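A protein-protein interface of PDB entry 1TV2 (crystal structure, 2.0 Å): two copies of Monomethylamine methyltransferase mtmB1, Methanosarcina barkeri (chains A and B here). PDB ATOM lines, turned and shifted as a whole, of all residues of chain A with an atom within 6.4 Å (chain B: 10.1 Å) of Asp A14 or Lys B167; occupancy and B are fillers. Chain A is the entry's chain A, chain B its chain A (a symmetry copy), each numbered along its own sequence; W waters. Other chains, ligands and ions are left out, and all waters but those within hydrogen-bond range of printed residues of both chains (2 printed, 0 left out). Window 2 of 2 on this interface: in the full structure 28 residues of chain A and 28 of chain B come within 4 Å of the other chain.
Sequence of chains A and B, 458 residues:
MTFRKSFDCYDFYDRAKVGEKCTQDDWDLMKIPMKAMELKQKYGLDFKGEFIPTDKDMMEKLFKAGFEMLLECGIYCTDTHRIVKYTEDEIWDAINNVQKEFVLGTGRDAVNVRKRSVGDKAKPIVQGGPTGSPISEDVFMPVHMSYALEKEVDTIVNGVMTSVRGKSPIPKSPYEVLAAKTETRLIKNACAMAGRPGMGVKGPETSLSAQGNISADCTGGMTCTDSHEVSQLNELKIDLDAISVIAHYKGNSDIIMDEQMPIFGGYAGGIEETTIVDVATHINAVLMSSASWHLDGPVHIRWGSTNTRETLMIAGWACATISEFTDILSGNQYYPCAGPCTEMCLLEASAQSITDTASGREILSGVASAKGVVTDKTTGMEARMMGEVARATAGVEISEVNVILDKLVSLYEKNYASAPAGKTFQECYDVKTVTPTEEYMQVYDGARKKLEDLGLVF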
ATOM      1  N   ARG A   4      15.344  25.590  39.815  1.00  0.00           N
ATOM      2  CA  ARG A   4      16.554  25.524  39.009  1.00  0.00           C
ATOM      3  C   ARG A   4      16.253  25.875  37.555  1.00  0.00           C
ATOM      4  O   ARG A   4      16.924  26.717  36.956  1.00  0.00           O
ATOM      5  CB  ARG A   4      17.169  24.127  39.090  1.00  0.00           C
ATOM      6  CG  ARG A   4      18.616  24.084  38.637  1.00  0.00           C
ATOM      7  CD  ARG A   4      19.228  22.701  38.786  1.00  0.00           C
ATOM      8  NE  ARG A   4      18.536  21.704  37.974  1.00  0.00           N
ATOM      9  CZ  ARG A   4      19.113  20.609  37.488  1.00  0.00           C
ATOM     10  NH1 ARG A   4      20.395  20.369  37.731  1.00  0.00           N
ATOM     11  NH2 ARG A   4      18.409  19.757  36.757  1.00  0.00           N
ATOM     12  N   CYS A   9       9.521  17.396  30.560  1.00  0.00           N
ATOM     13  CA  CYS A   9       9.616  15.947  30.432  1.00  0.00           C
ATOM     14  C   CYS A   9      11.030  15.418  30.672  1.00  0.00           C
ATOM     15  O   CYS A   9      11.204  14.286  31.129  1.00  0.00           O
ATOM     16  CB  CYS A   9       9.135  15.525  29.039  1.00  0.00           C
ATOM     17  SG  CYS A   9      10.005  16.339  27.665  1.00  0.00           S
ATOM     18  N   TYR A  10      12.035  16.230  30.361  1.00  0.00           N
ATOM     19  CA  TYR A  10      13.421  15.813  30.554  1.00  0.00           C
ATOM     20  C   TYR A  10      13.765  15.736  32.040  1.00  0.00           C
ATOM     21  O   TYR A  10      14.440  14.807  32.480  1.00  0.00           O
ATOM     22  CB  TYR A  10      14.367  16.771  29.823  1.00  0.00           C
ATOM     23  CG  TYR A  10      14.090  16.827  28.336  1.00  0.00           C
ATOM     24  CD1 TYR A  10      13.363  17.879  27.777  1.00  0.00           C
ATOM     25  CD2 TYR A  10      14.497  15.791  27.498  1.00  0.00           C
ATOM     26  CE1 TYR A  10      13.043  17.893  26.417  1.00  0.00           C
ATOM     27  CE2 TYR A  10      14.185  15.794  26.138  1.00  0.00           C
ATOM     28  CZ  TYR A  10      13.457  16.845  25.606  1.00  0.00           C
ATOM     29  OH  TYR A  10      13.136  16.839  24.269  1.00  0.00           O
ATOM     30  N   ASP A  11      13.294  16.709  32.813  1.00  0.00           N
ATOM     31  CA  ASP A  11      13.541  16.709  34.250  1.00  0.00           C
ATOM     32  C   ASP A  11      12.787  15.536  34.865  1.00  0.00           C
ATOM     33  O   ASP A  11      13.261  14.901  35.808  1.00  0.00           O
ATOM     34  CB  ASP A  11      13.055  18.011  34.882  1.00  0.00           C
ATOM     35  CG  ASP A  11      13.746  19.228  34.307  1.00  0.00           C
ATOM     36  OD1 ASP A  11      14.993  19.274  34.343  1.00  0.00           O
ATOM     37  OD2 ASP A  11      13.040  20.137  33.821  1.00  0.00           O
ATOM     38  N   PHE A  12      11.608  15.247  34.325  1.00  0.00           N
ATOM     39  CA  PHE A  12      10.817  14.147  34.841  1.00  0.00           C
ATOM     40  C   PHE A  12      11.587  12.838  34.716  1.00  0.00           C
ATOM     41  O   PHE A  12      11.668  12.066  35.671  1.00  0.00           O
ATOM     42  CB  PHE A  12       9.492  14.018  34.096  1.00  0.00           C
ATOM     43  CG  PHE A  12       8.524  13.106  34.780  1.00  0.00           C
ATOM     44  CD1 PHE A  12       7.605  13.609  35.696  1.00  0.00           C
ATOM     45  CD2 PHE A  12       8.587  11.730  34.578  1.00  0.00           C
ATOM     46  CE1 PHE A  12       6.766  12.755  36.407  1.00  0.00           C
ATOM     47  CE2 PHE A  12       7.753  10.866  35.285  1.00  0.00           C
ATOM     48  CZ  PHE A  12       6.842  11.381  36.202  1.00  0.00           C
ATOM     49  N   TYR A  13      12.148  12.586  33.536  1.00  0.00           N
ATOM     50  CA  TYR A  13      12.915  11.365  33.310  1.00  0.00           C
ATOM     51  C   TYR A  13      14.067  11.285  34.310  1.00  0.00           C
ATOM     52  O   TYR A  13      14.279  10.252  34.947  1.00  0.00           O
ATOM     53  CB  TYR A  13      13.474  11.337  31.886  1.00  0.00           C
ATOM     54  CG  TYR A  13      14.322  10.117  31.596  1.00  0.00           C
ATOM     55  CD1 TYR A  13      13.737   8.872  31.369  1.00  0.00           C
ATOM     56  CD2 TYR A  13      15.714  10.203  31.576  1.00  0.00           C
ATOM     57  CE1 TYR A  13      14.519   7.741  31.127  1.00  0.00           C
ATOM     58  CE2 TYR A  13      16.507   9.080  31.337  1.00  0.00           C
ATOM     59  CZ  TYR A  13      15.904   7.856  31.113  1.00  0.00           C
ATOM     60  OH  TYR A  13      16.686   6.750  30.871  1.00  0.00           O
ATOM     61  N   ASP A  14      14.814  12.378  34.437  1.00  0.00           N
ATOM     62  CA  ASP A  14      15.940  12.428  35.364  1.00  0.00           C
ATOM     63  C   ASP A  14      15.510  11.980  36.764  1.00  0.00           C
ATOM     64  O   ASP A  14      16.097  11.065  37.346  1.00  0.00           O
ATOM     65  CB  ASP A  14      16.502  13.853  35.450  1.00  0.00           C
ATOM     66  CG  ASP A  14      17.250  14.272  34.195  1.00  0.00           C
ATOM     67  OD1 ASP A  14      17.638  15.457  34.113  1.00  0.00           O
ATOM     68  OD2 ASP A  14      17.463  13.428  33.299  1.00  0.00           O
ATOM     69  N   ARG A  15      14.474  12.621  37.291  1.00  0.00           N
ATOM     70  CA  ARG A  15      13.978  12.311  38.630  1.00  0.00           C
ATOM     71  C   ARG A  15      13.352  10.926  38.774  1.00  0.00           C
ATOM     72  O   ARG A  15      13.493  10.285  39.818  1.00  0.00           O
ATOM     73  CB  ARG A  15      12.983  13.391  39.068  1.00  0.00           C
ATOM     74  CG  ARG A  15      13.580  14.788  38.994  1.00  0.00           C
ATOM     75  CD  ARG A  15      12.646  15.870  39.514  1.00  0.00           C
ATOM     76  NE  ARG A  15      13.243  17.191  39.327  1.00  0.00           N
ATOM     77  CZ  ARG A  15      12.696  18.337  39.724  1.00  0.00           C
ATOM     78  NH1 ARG A  15      11.522  18.344  40.344  1.00  0.00           N
ATOM     79  NH2 ARG A  15      13.325  19.482  39.485  1.00  0.00           N
ATOM     80  N   ALA A  16      12.667  10.463  37.733  1.00  0.00           N
ATOM     81  CA  ALA A  16      12.020   9.155  37.759  1.00  0.00           C
ATOM     82  C   ALA A  16      13.021   8.013  37.924  1.00  0.00           C
ATOM     83  O   ALA A  16      12.658   6.917  38.352  1.00  0.00           O
ATOM     84  CB  ALA A  16      11.209   8.947  36.484  1.00  0.00           C
ATOM     85  N   LYS A  17      14.277   8.273  37.577  1.00  0.00           N
ATOM     86  CA  LYS A  17      15.319   7.256  37.676  1.00  0.00           C
ATOM     87  C   LYS A  17      15.899   7.138  39.081  1.00  0.00           C
ATOM     88  O   LYS A  17      16.360   6.066  39.475  1.00  0.00           O
ATOM     89  CB  LYS A  17      16.459   7.565  36.695  1.00  0.00           C
ATOM     90  CG  LYS A  17      16.043   7.619  35.237  1.00  0.00           C
ATOM     91  CD  LYS A  17      15.599   6.258  34.724  1.00  0.00           C
ATOM     92  CE  LYS A  17      16.786   5.332  34.514  1.00  0.00           C
ATOM     93  NZ  LYS A  17      17.737   5.874  33.498  1.00  0.00           N
ATOM     94  N   VAL A  18      15.867   8.232  39.835  1.00  0.00           N
ATOM     95  CA  VAL A  18      16.434   8.240  41.180  1.00  0.00           C
ATOM     96  C   VAL A  18      15.458   8.615  42.292  1.00  0.00           C
ATOM     97  O   VAL A  18      15.869   8.839  43.431  1.00  0.00           O
ATOM     98  CB  VAL A  18      17.631   9.208  41.250  1.00  0.00           C
ATOM     99  CG1 VAL A  18      18.672   8.817  40.205  1.00  0.00           C
ATOM    100  CG2 VAL A  18      17.162  10.638  41.011  1.00  0.00           C
ATOM    101  N   GLY A  19      14.172   8.682  41.968  1.00  0.00           N
ATOM    102  CA  GLY A  19      13.187   9.042  42.971  1.00  0.00           C
ATOM    103  C   GLY A  19      12.975   7.969  44.025  1.00  0.00           C
ATOM    104  O   GLY A  19      13.559   6.886  43.952  1.00  0.00           O
ATOM    105  N   ILE B 135      30.811  11.828  19.157  1.00  0.00           N
ATOM    106  CA  ILE B 135      31.346  13.182  19.110  1.00  0.00           C
ATOM    107  C   ILE B 135      30.842  13.976  20.312  1.00  0.00           C
ATOM    108  O   ILE B 135      29.650  13.956  20.616  1.00  0.00           O
ATOM    109  CB  ILE B 135      30.903  13.912  17.817  1.00  0.00           C
ATOM    110  CG1 ILE B 135      31.333  13.104  16.584  1.00  0.00           C
ATOM    111  CG2 ILE B 135      31.486  15.318  17.784  1.00  0.00           C
ATOM    112  CD1 ILE B 135      32.828  12.904  16.453  1.00  0.00           C
ATOM    113  N   SER B 136      31.754  14.668  20.991  1.00  0.00           N
ATOM    114  CA  SER B 136      31.399  15.477  22.153  1.00  0.00           C
ATOM    115  C   SER B 136      30.397  16.556  21.755  1.00  0.00           C
ATOM    116  O   SER B 136      30.504  17.156  20.682  1.00  0.00           O
ATOM    117  CB  SER B 136      32.647  16.134  22.747  1.00  0.00           C
ATOM    118  OG  SER B 136      33.598  15.161  23.143  1.00  0.00           O
ATOM    119  N   GLU B 137      29.433  16.813  22.630  1.00  0.00           N
ATOM    120  CA  GLU B 137      28.412  17.808  22.345  1.00  0.00           C
ATOM    121  C   GLU B 137      28.971  19.199  22.044  1.00  0.00           C
ATOM    122  O   GLU B 137      28.505  19.865  21.117  1.00  0.00           O
ATOM    123  CB  GLU B 137      27.419  17.901  23.508  1.00  0.00           C
ATOM    124  CG  GLU B 137      26.228  18.804  23.210  1.00  0.00           C
ATOM    125  CD  GLU B 137      25.186  18.823  24.319  1.00  0.00           C
ATOM    126  OE1 GLU B 137      24.163  19.525  24.154  1.00  0.00           O
ATOM    127  OE2 GLU B 137      25.383  18.136  25.348  1.00  0.00           O
ATOM    128  N   ASP B 138      29.975  19.634  22.802  1.00  0.00           N
ATOM    129  CA  ASP B 138      30.522  20.971  22.595  1.00  0.00           C
ATOM    130  C   ASP B 138      31.260  21.213  21.275  1.00  0.00           C
ATOM    131  O   ASP B 138      31.577  22.356  20.945  1.00  0.00           O
ATOM    132  CB  ASP B 138      31.401  21.383  23.787  1.00  0.00           C
ATOM    133  CG  ASP B 138      32.641  20.525  23.938  1.00  0.00           C
ATOM    134  OD1 ASP B 138      32.802  19.532  23.198  1.00  0.00           O
ATOM    135  OD2 ASP B 138      33.463  20.852  24.818  1.00  0.00           O
ATOM    136  N   VAL B 160      27.544  10.643  16.144  1.00  0.00           N
ATOM    137  CA  VAL B 160      26.649  10.405  17.272  1.00  0.00           C
ATOM    138  C   VAL B 160      26.914  11.394  18.406  1.00  0.00           C
ATOM    139  O   VAL B 160      28.065  11.614  18.780  1.00  0.00           O
ATOM    140  CB  VAL B 160      26.833   8.961  17.808  1.00  0.00           C
ATOM    141  CG1 VAL B 160      26.217   8.826  19.193  1.00  0.00           C
ATOM    142  CG2 VAL B 160      26.197   7.969  16.840  1.00  0.00           C
ATOM    143  N   MET B 161      25.853  11.987  18.949  1.00  0.00           N
ATOM    144  CA  MET B 161      25.992  12.939  20.054  1.00  0.00           C
ATOM    145  C   MET B 161      26.235  12.158  21.344  1.00  0.00           C
ATOM    146  O   MET B 161      25.391  11.355  21.743  1.00  0.00           O
ATOM    147  CB  MET B 161      24.715  13.776  20.219  1.00  0.00           C
ATOM    148  CG  MET B 161      24.356  14.673  19.032  1.00  0.00           C
ATOM    149  SD  MET B 161      22.916  15.733  19.367  1.00  0.00           S
ATOM    150  CE  MET B 161      23.666  17.019  20.396  1.00  0.00           C
ATOM    151  N   THR B 162      27.375  12.376  21.999  1.00  0.00           N
ATOM    152  CA  THR B 162      27.645  11.662  23.245  1.00  0.00           C
ATOM    153  C   THR B 162      26.684  12.164  24.316  1.00  0.00           C
ATOM    154  O   THR B 162      26.396  11.461  25.281  1.00  0.00           O
ATOM    155  CB  THR B 162      29.109  11.836  23.719  1.00  0.00           C
ATOM    156  OG1 THR B 162      29.421  13.228  23.846  1.00  0.00           O
ATOM    157  CG2 THR B 162      30.063  11.181  22.727  1.00  0.00           C
ATOM    158  N   SER B 163      26.186  13.385  24.139  1.00  0.00           N
ATOM    159  CA  SER B 163      25.211  13.964  25.060  1.00  0.00           C
ATOM    160  C   SER B 163      24.435  15.083  24.374  1.00  0.00           C
ATOM    161  O   SER B 163      24.891  15.663  23.388  1.00  0.00           O
ATOM    162  CB  SER B 163      25.886  14.528  26.317  1.00  0.00           C
ATOM    163  OG  SER B 163      26.571  15.745  26.045  1.00  0.00           O
ATOM    164  N   VAL B 164      23.248  15.360  24.895  1.00  0.00           N
ATOM    165  CA  VAL B 164      22.417  16.438  24.389  1.00  0.00           C
ATOM    166  C   VAL B 164      21.934  17.136  25.658  1.00  0.00           C
ATOM    167  O   VAL B 164      21.359  16.503  26.548  1.00  0.00           O
ATOM    168  CB  VAL B 164      21.237  15.910  23.522  1.00  0.00           C
ATOM    169  CG1 VAL B 164      20.323  15.004  24.333  1.00  0.00           C
ATOM    170  CG2 VAL B 164      20.470  17.088  22.940  1.00  0.00           C
ATOM    171  N   ARG B 165      22.202  18.435  25.752  1.00  0.00           N
ATOM    172  CA  ARG B 165      21.855  19.206  26.939  1.00  0.00           C
ATOM    173  C   ARG B 165      22.523  18.573  28.162  1.00  0.00           C
ATOM    174  O   ARG B 165      21.954  18.524  29.252  1.00  0.00           O
ATOM    175  CB  ARG B 165      20.333  19.294  27.115  1.00  0.00           C
ATOM    176  CG  ARG B 165      19.746  20.535  26.433  1.00  0.00           C
ATOM    177  CD  ARG B 165      18.226  20.534  26.380  1.00  0.00           C
ATOM    178  NE  ARG B 165      17.609  20.555  27.701  1.00  0.00           N
ATOM    179  CZ  ARG B 165      16.298  20.620  27.902  1.00  0.00           C
ATOM    180  NH1 ARG B 165      15.470  20.674  26.867  1.00  0.00           N
ATOM    181  NH2 ARG B 165      15.810  20.615  29.135  1.00  0.00           N
ATOM    182  N   GLY B 166      23.742  18.081  27.948  1.00  0.00           N
ATOM    183  CA  GLY B 166      24.524  17.475  29.014  1.00  0.00           C
ATOM    184  C   GLY B 166      24.096  16.107  29.513  1.00  0.00           C
ATOM    185  O   GLY B 166      24.611  15.636  30.528  1.00  0.00           O
ATOM    186  N   LYS B 167      23.178  15.455  28.807  1.00  0.00           N
ATOM    187  CA  LYS B 167      22.692  14.139  29.223  1.00  0.00           C
ATOM    188  C   LYS B 167      22.850  13.091  28.128  1.00  0.00           C
ATOM    189  O   LYS B 167      22.774  13.407  26.941  1.00  0.00           O
ATOM    190  CB  LYS B 167      21.216  14.234  29.605  1.00  0.00           C
ATOM    191  CG  LYS B 167      20.921  15.178  30.756  1.00  0.00           C
ATOM    192  CD  LYS B 167      21.347  14.571  32.076  1.00  0.00           C
ATOM    193  CE  LYS B 167      20.982  15.478  33.229  1.00  0.00           C
ATOM    194  NZ  LYS B 167      21.315  14.840  34.529  1.00  0.00           N
ATOM    195  N   SER B 168      23.055  11.838  28.531  1.00  0.00           N
ATOM    196  CA  SER B 168      23.198  10.750  27.568  1.00  0.00           C
ATOM    197  C   SER B 168      21.849  10.463  26.919  1.00  0.00           C
ATOM    198  O   SER B 168      20.830  10.373  27.601  1.00  0.00           O
ATOM    199  CB  SER B 168      23.711   9.480  28.257  1.00  0.00           C
ATOM    200  OG  SER B 168      25.007   9.683  28.790  1.00  0.00           O
ATOM    201  N   PRO B 169      21.822  10.327  25.584  1.00  0.00           N
ATOM    202  CA  PRO B 169      20.579  10.048  24.859  1.00  0.00           C
ATOM    203  C   PRO B 169      20.163   8.584  25.015  1.00  0.00           C
ATOM    204  O   PRO B 169      20.039   7.857  24.034  1.00  0.00           O
ATOM    205  CB  PRO B 169      20.942  10.400  23.424  1.00  0.00           C
ATOM    206  CG  PRO B 169      22.380   9.968  23.341  1.00  0.00           C
ATOM    207  CD  PRO B 169      22.954  10.492  24.651  1.00  0.00           C
ATOM    208  N   ILE B 170      19.954   8.162  26.257  1.00  0.00           N
ATOM    209  CA  ILE B 170      19.577   6.781  26.554  1.00  0.00           C
ATOM    210  C   ILE B 170      18.377   6.305  25.742  1.00  0.00           C
ATOM    211  O   ILE B 170      17.353   6.981  25.671  1.00  0.00           O
ATOM    212  CB  ILE B 170      19.266   6.611  28.058  1.00  0.00           C
ATOM    213  CG1 ILE B 170      20.504   6.967  28.882  1.00  0.00           C
ATOM    214  CG2 ILE B 170      18.821   5.178  28.344  1.00  0.00           C
ATOM    215  CD1 ILE B 170      20.246   7.031  30.371  1.00  0.00           C
ATOM    216  N   PRO B 171      18.491   5.121  25.118  1.00  0.00           N
ATOM    217  CA  PRO B 171      17.389   4.583  24.317  1.00  0.00           C
ATOM    218  C   PRO B 171      16.074   4.576  25.089  1.00  0.00           C
ATOM    219  O   PRO B 171      16.032   4.210  26.263  1.00  0.00           O
ATOM    220  CB  PRO B 171      17.872   3.180  23.968  1.00  0.00           C
ATOM    221  CG  PRO B 171      19.352   3.366  23.859  1.00  0.00           C
ATOM    222  CD  PRO B 171      19.657   4.223  25.069  1.00  0.00           C
ATOM    223  N   SER B 173      14.404   7.060  26.144  1.00  0.00           N
ATOM    224  CA  SER B 173      14.303   8.153  27.106  1.00  0.00           C
ATOM    225  C   SER B 173      13.953   9.374  26.253  1.00  0.00           C
ATOM    226  O   SER B 173      14.167   9.363  25.038  1.00  0.00           O
ATOM    227  CB  SER B 173      15.644   8.398  27.804  1.00  0.00           C
ATOM    228  OG  SER B 173      16.554   9.064  26.938  1.00  0.00           O
ATOM    229  N   PRO B 174      13.398  10.433  26.864  1.00  0.00           N
ATOM    230  CA  PRO B 174      13.068  11.605  26.047  1.00  0.00           C
ATOM    231  C   PRO B 174      14.319  12.215  25.407  1.00  0.00           C
ATOM    232  O   PRO B 174      14.242  12.845  24.353  1.00  0.00           O
ATOM    233  CB  PRO B 174      12.393  12.548  27.044  1.00  0.00           C
ATOM    234  CG  PRO B 174      13.007  12.142  28.374  1.00  0.00           C
ATOM    235  CD  PRO B 174      13.013  10.640  28.271  1.00  0.00           C
ATOM    236  N   TYR B 175      15.471  12.014  26.042  1.00  0.00           N
ATOM    237  CA  TYR B 175      16.722  12.541  25.510  1.00  0.00           C
ATOM    238  C   TYR B 175      17.087  11.905  24.171  1.00  0.00           C
ATOM    239  O   TYR B 175      17.754  12.532  23.350  1.00  0.00           O
ATOM    240  CB  TYR B 175      17.870  12.335  26.502  1.00  0.00           C
ATOM    241  CG  TYR B 175      17.767  13.202  27.735  1.00  0.00           C
ATOM    242  CD1 TYR B 175      17.347  12.667  28.953  1.00  0.00           C
ATOM    243  CD2 TYR B 175      18.081  14.562  27.682  1.00  0.00           C
ATOM    244  CE1 TYR B 175      17.243  13.463  30.091  1.00  0.00           C
ATOM    245  CE2 TYR B 175      17.979  15.366  28.813  1.00  0.00           C
ATOM    246  CZ  TYR B 175      17.561  14.808  30.013  1.00  0.00           C
ATOM    247  OH  TYR B 175      17.462  15.588  31.138  1.00  0.00           O
ATOM    248  N   GLU B 176      16.656  10.665  23.949  1.00  0.00           N
ATOM    249  CA  GLU B 176      16.952  10.001  22.682  1.00  0.00           C
ATOM    250  C   GLU B 176      16.170  10.693  21.568  1.00  0.00           C
ATOM    251  O   GLU B 176      16.685  10.888  20.468  1.00  0.00           O
ATOM    252  CB  GLU B 176      16.575   8.515  22.720  1.00  0.00           C
ATOM    253  CG  GLU B 176      16.729   7.842  21.353  1.00  0.00           C
ATOM    254  CD  GLU B 176      16.270   6.395  21.328  1.00  0.00           C
ATOM    255  OE1 GLU B 176      15.209   6.096  21.914  1.00  0.00           O
ATOM    256  OE2 GLU B 176      16.962   5.566  20.701  1.00  0.00           O
ATOM    257  N   VAL B 177      14.920  11.052  21.855  1.00  0.00           N
ATOM    258  CA  VAL B 177      14.078  11.742  20.879  1.00  0.00           C
ATOM    259  C   VAL B 177      14.688  13.111  20.588  1.00  0.00           C
ATOM    260  O   VAL B 177      14.812  13.512  19.430  1.00  0.00           O
ATOM    261  CB  VAL B 177      12.632  11.925  21.413  1.00  0.00           C
ATOM    262  CG1 VAL B 177      11.870  12.936  20.563  1.00  0.00           C
ATOM    263  CG2 VAL B 177      11.904  10.583  21.389  1.00  0.00           C
ATOM    264  N   LEU B 178      15.079  13.818  21.645  1.00  0.00           N
ATOM    265  CA  LEU B 178      15.683  15.138  21.497  1.00  0.00           C
ATOM    266  C   LEU B 178      16.924  15.071  20.611  1.00  0.00           C
ATOM    267  O   LEU B 178      17.106  15.905  19.720  1.00  0.00           O
ATOM    268  CB  LEU B 178      16.066  15.708  22.868  1.00  0.00           C
ATOM    269  CG  LEU B 178      16.752  17.080  22.842  1.00  0.00           C
ATOM    270  CD1 LEU B 178      15.825  18.116  22.197  1.00  0.00           C
ATOM    271  CD2 LEU B 178      17.115  17.495  24.262  1.00  0.00           C
ATOM    272  N   ALA B 179      17.772  14.075  20.857  1.00  0.00           N
ATOM    273  CA  ALA B 179      18.998  13.899  20.085  1.00  0.00           C
ATOM    274  C   ALA B 179      18.719  13.543  18.631  1.00  0.00           C
ATOM    275  O   ALA B 179      19.405  14.023  17.729  1.00  0.00           O
ATOM    276  CB  ALA B 179      19.874  12.825  20.727  1.00  0.00           C
ATOM    277  N   ALA B 180      17.717  12.696  18.400  1.00  0.00           N
ATOM    278  CA  ALA B 180      17.365  12.290  17.043  1.00  0.00           C
ATOM    279  C   ALA B 180      16.989  13.500  16.183  1.00  0.00           C
ATOM    280  O   ALA B 180      17.355  13.574  15.012  1.00  0.00           O
ATOM    281  CB  ALA B 180      16.210  11.294  17.072  1.00  0.00           C
ATOM    282  N   THR B 182      17.643  16.863  17.107  1.00  0.00           N
ATOM    283  CA  THR B 182      18.740  17.826  17.220  1.00  0.00           C
ATOM    284  C   THR B 182      19.947  17.498  16.347  1.00  0.00           C
ATOM    285  O   THR B 182      20.547  18.379  15.727  1.00  0.00           O
ATOM    286  CB  THR B 182      19.209  17.936  18.690  1.00  0.00           C
ATOM    287  OG1 THR B 182      18.096  18.303  19.516  1.00  0.00           O
ATOM    288  CG2 THR B 182      20.302  18.985  18.834  1.00  0.00           C
ATOM    289  N   THR B 206      22.283   8.917  16.377  1.00  0.00           N
ATOM    290  CA  THR B 206      22.264   8.882  17.839  1.00  0.00           C
ATOM    291  C   THR B 206      21.152   8.001  18.415  1.00  0.00           C
ATOM    292  O   THR B 206      21.330   7.375  19.462  1.00  0.00           O
ATOM    293  CB  THR B 206      22.149  10.311  18.419  1.00  0.00           C
ATOM    294  OG1 THR B 206      23.217  11.117  17.902  1.00  0.00           O
ATOM    295  CG2 THR B 206      22.244  10.286  19.941  1.00  0.00           C
HETATM  296  O   HOH W   1      15.204   4.836  29.080  1.00  0.00           O
HETATM  297  O   HOH W   2      16.072  19.468  31.853  1.00  0.00           O
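No position is printed for both chains. Of the 11 pairs that touch across the chains among the printed residues, none has its exchanged pair printed and touching as well.
The side-chain hydroxyl (OH) of Tyr A13 sits at hydrogen-bond distance from the side-chain amino group (NZ) of Lys A17, at 3.0 Å. OE1 of Glu B137 is in hydrogen-bond range of N of Arg B165, at 2.8 Å. The side-chain hydroxyl of Ser B173 is in hydrogen-bond range of the backbone carbonyl oxygen of Ile B170 (2.6 Å). The backbone NH (N) of Tyr B175 sits close to the side-chain hydroxyl (OG) of Ser B173 (3.3 Å). The side-chain hydroxyl (OG) of Ser B173 sits at hydrogen-bond distance from the backbone NH (N) of Glu B176 (3.4 Å). O of Leu B178 lies within hydrogen-bond range of OG1 of Thr B182, at 2.6 Å.
Water W2 lies within hydrogen-bond range of the side-chain carboxylate (OD1) of Asp A11 and the guanidinium group (NH2) of Arg B165. Water W1 lies within hydrogen-bond range of the backbone carbonyl oxygen (O) of Pro B171 and the side-chain hydroxyl (OH) of Tyr A13.
The backbone carbonyl oxygen (O) of Tyr A10 sits at hydrogen-bond distance from the side-chain hydroxyl (OH) of Tyr B175, at 3.4 Å. OD1 of Asp A14 is in salt-bridge range of NZ of Lys B167 (3.8 Å). The side-chain carboxylate of Asp A14 lies within hydrogen-bond range of the side-chain hydroxyl of Tyr B175 (3.0 Å).
Hydrophobic or aromatic side chains of chain B that line the printed part of chain A: Ile B170, Pro B174, Tyr B175 and Leu B178.
Cys A9 touches Pro B174. Arg B165 touches Tyr A10 (NH1 to CD1, 3.6 Å). Pro B174 touches Tyr A10. Tyr A10 touches Leu B178 (OH to CB, 3.4 Å). Tyr A13 touches Ile B170. Tyr A13 touches Ser B173 (CZ to CB, 3.4 Å). CG of Tyr A13 touches CD of Pro B174 (3.6 Å). Tyr A13 touches Tyr B175.
Of the printed residues of chain B, Tyr A10 touches Arg B165, Pro B174, Tyr B175 and Leu B178. Printed residues of chain B within 4 Å of Tyr A13: Ile B170, Ser B173, Pro B174 and Tyr B175. Asp A14 touches just these residues of chain B: Lys B167 and Tyr B175. Ala A16 touches none of the printed residues of chain B. Of the printed residues of chain A, Ser B173 touches Tyr A13. Of the printed residues of chain A, Tyr B175 touches Tyr A10, Tyr A13 and Asp A14. Printed residues of chain A within 4 Å of Leu B178: Tyr A10 (3.4 Å). The nearest residue of chain B that does not touch Asp A14 is Pro B174 (6.3 Å). The nearest printed residue of chain A that does not touch Ser B173 is Tyr A10 (6.4 Å).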
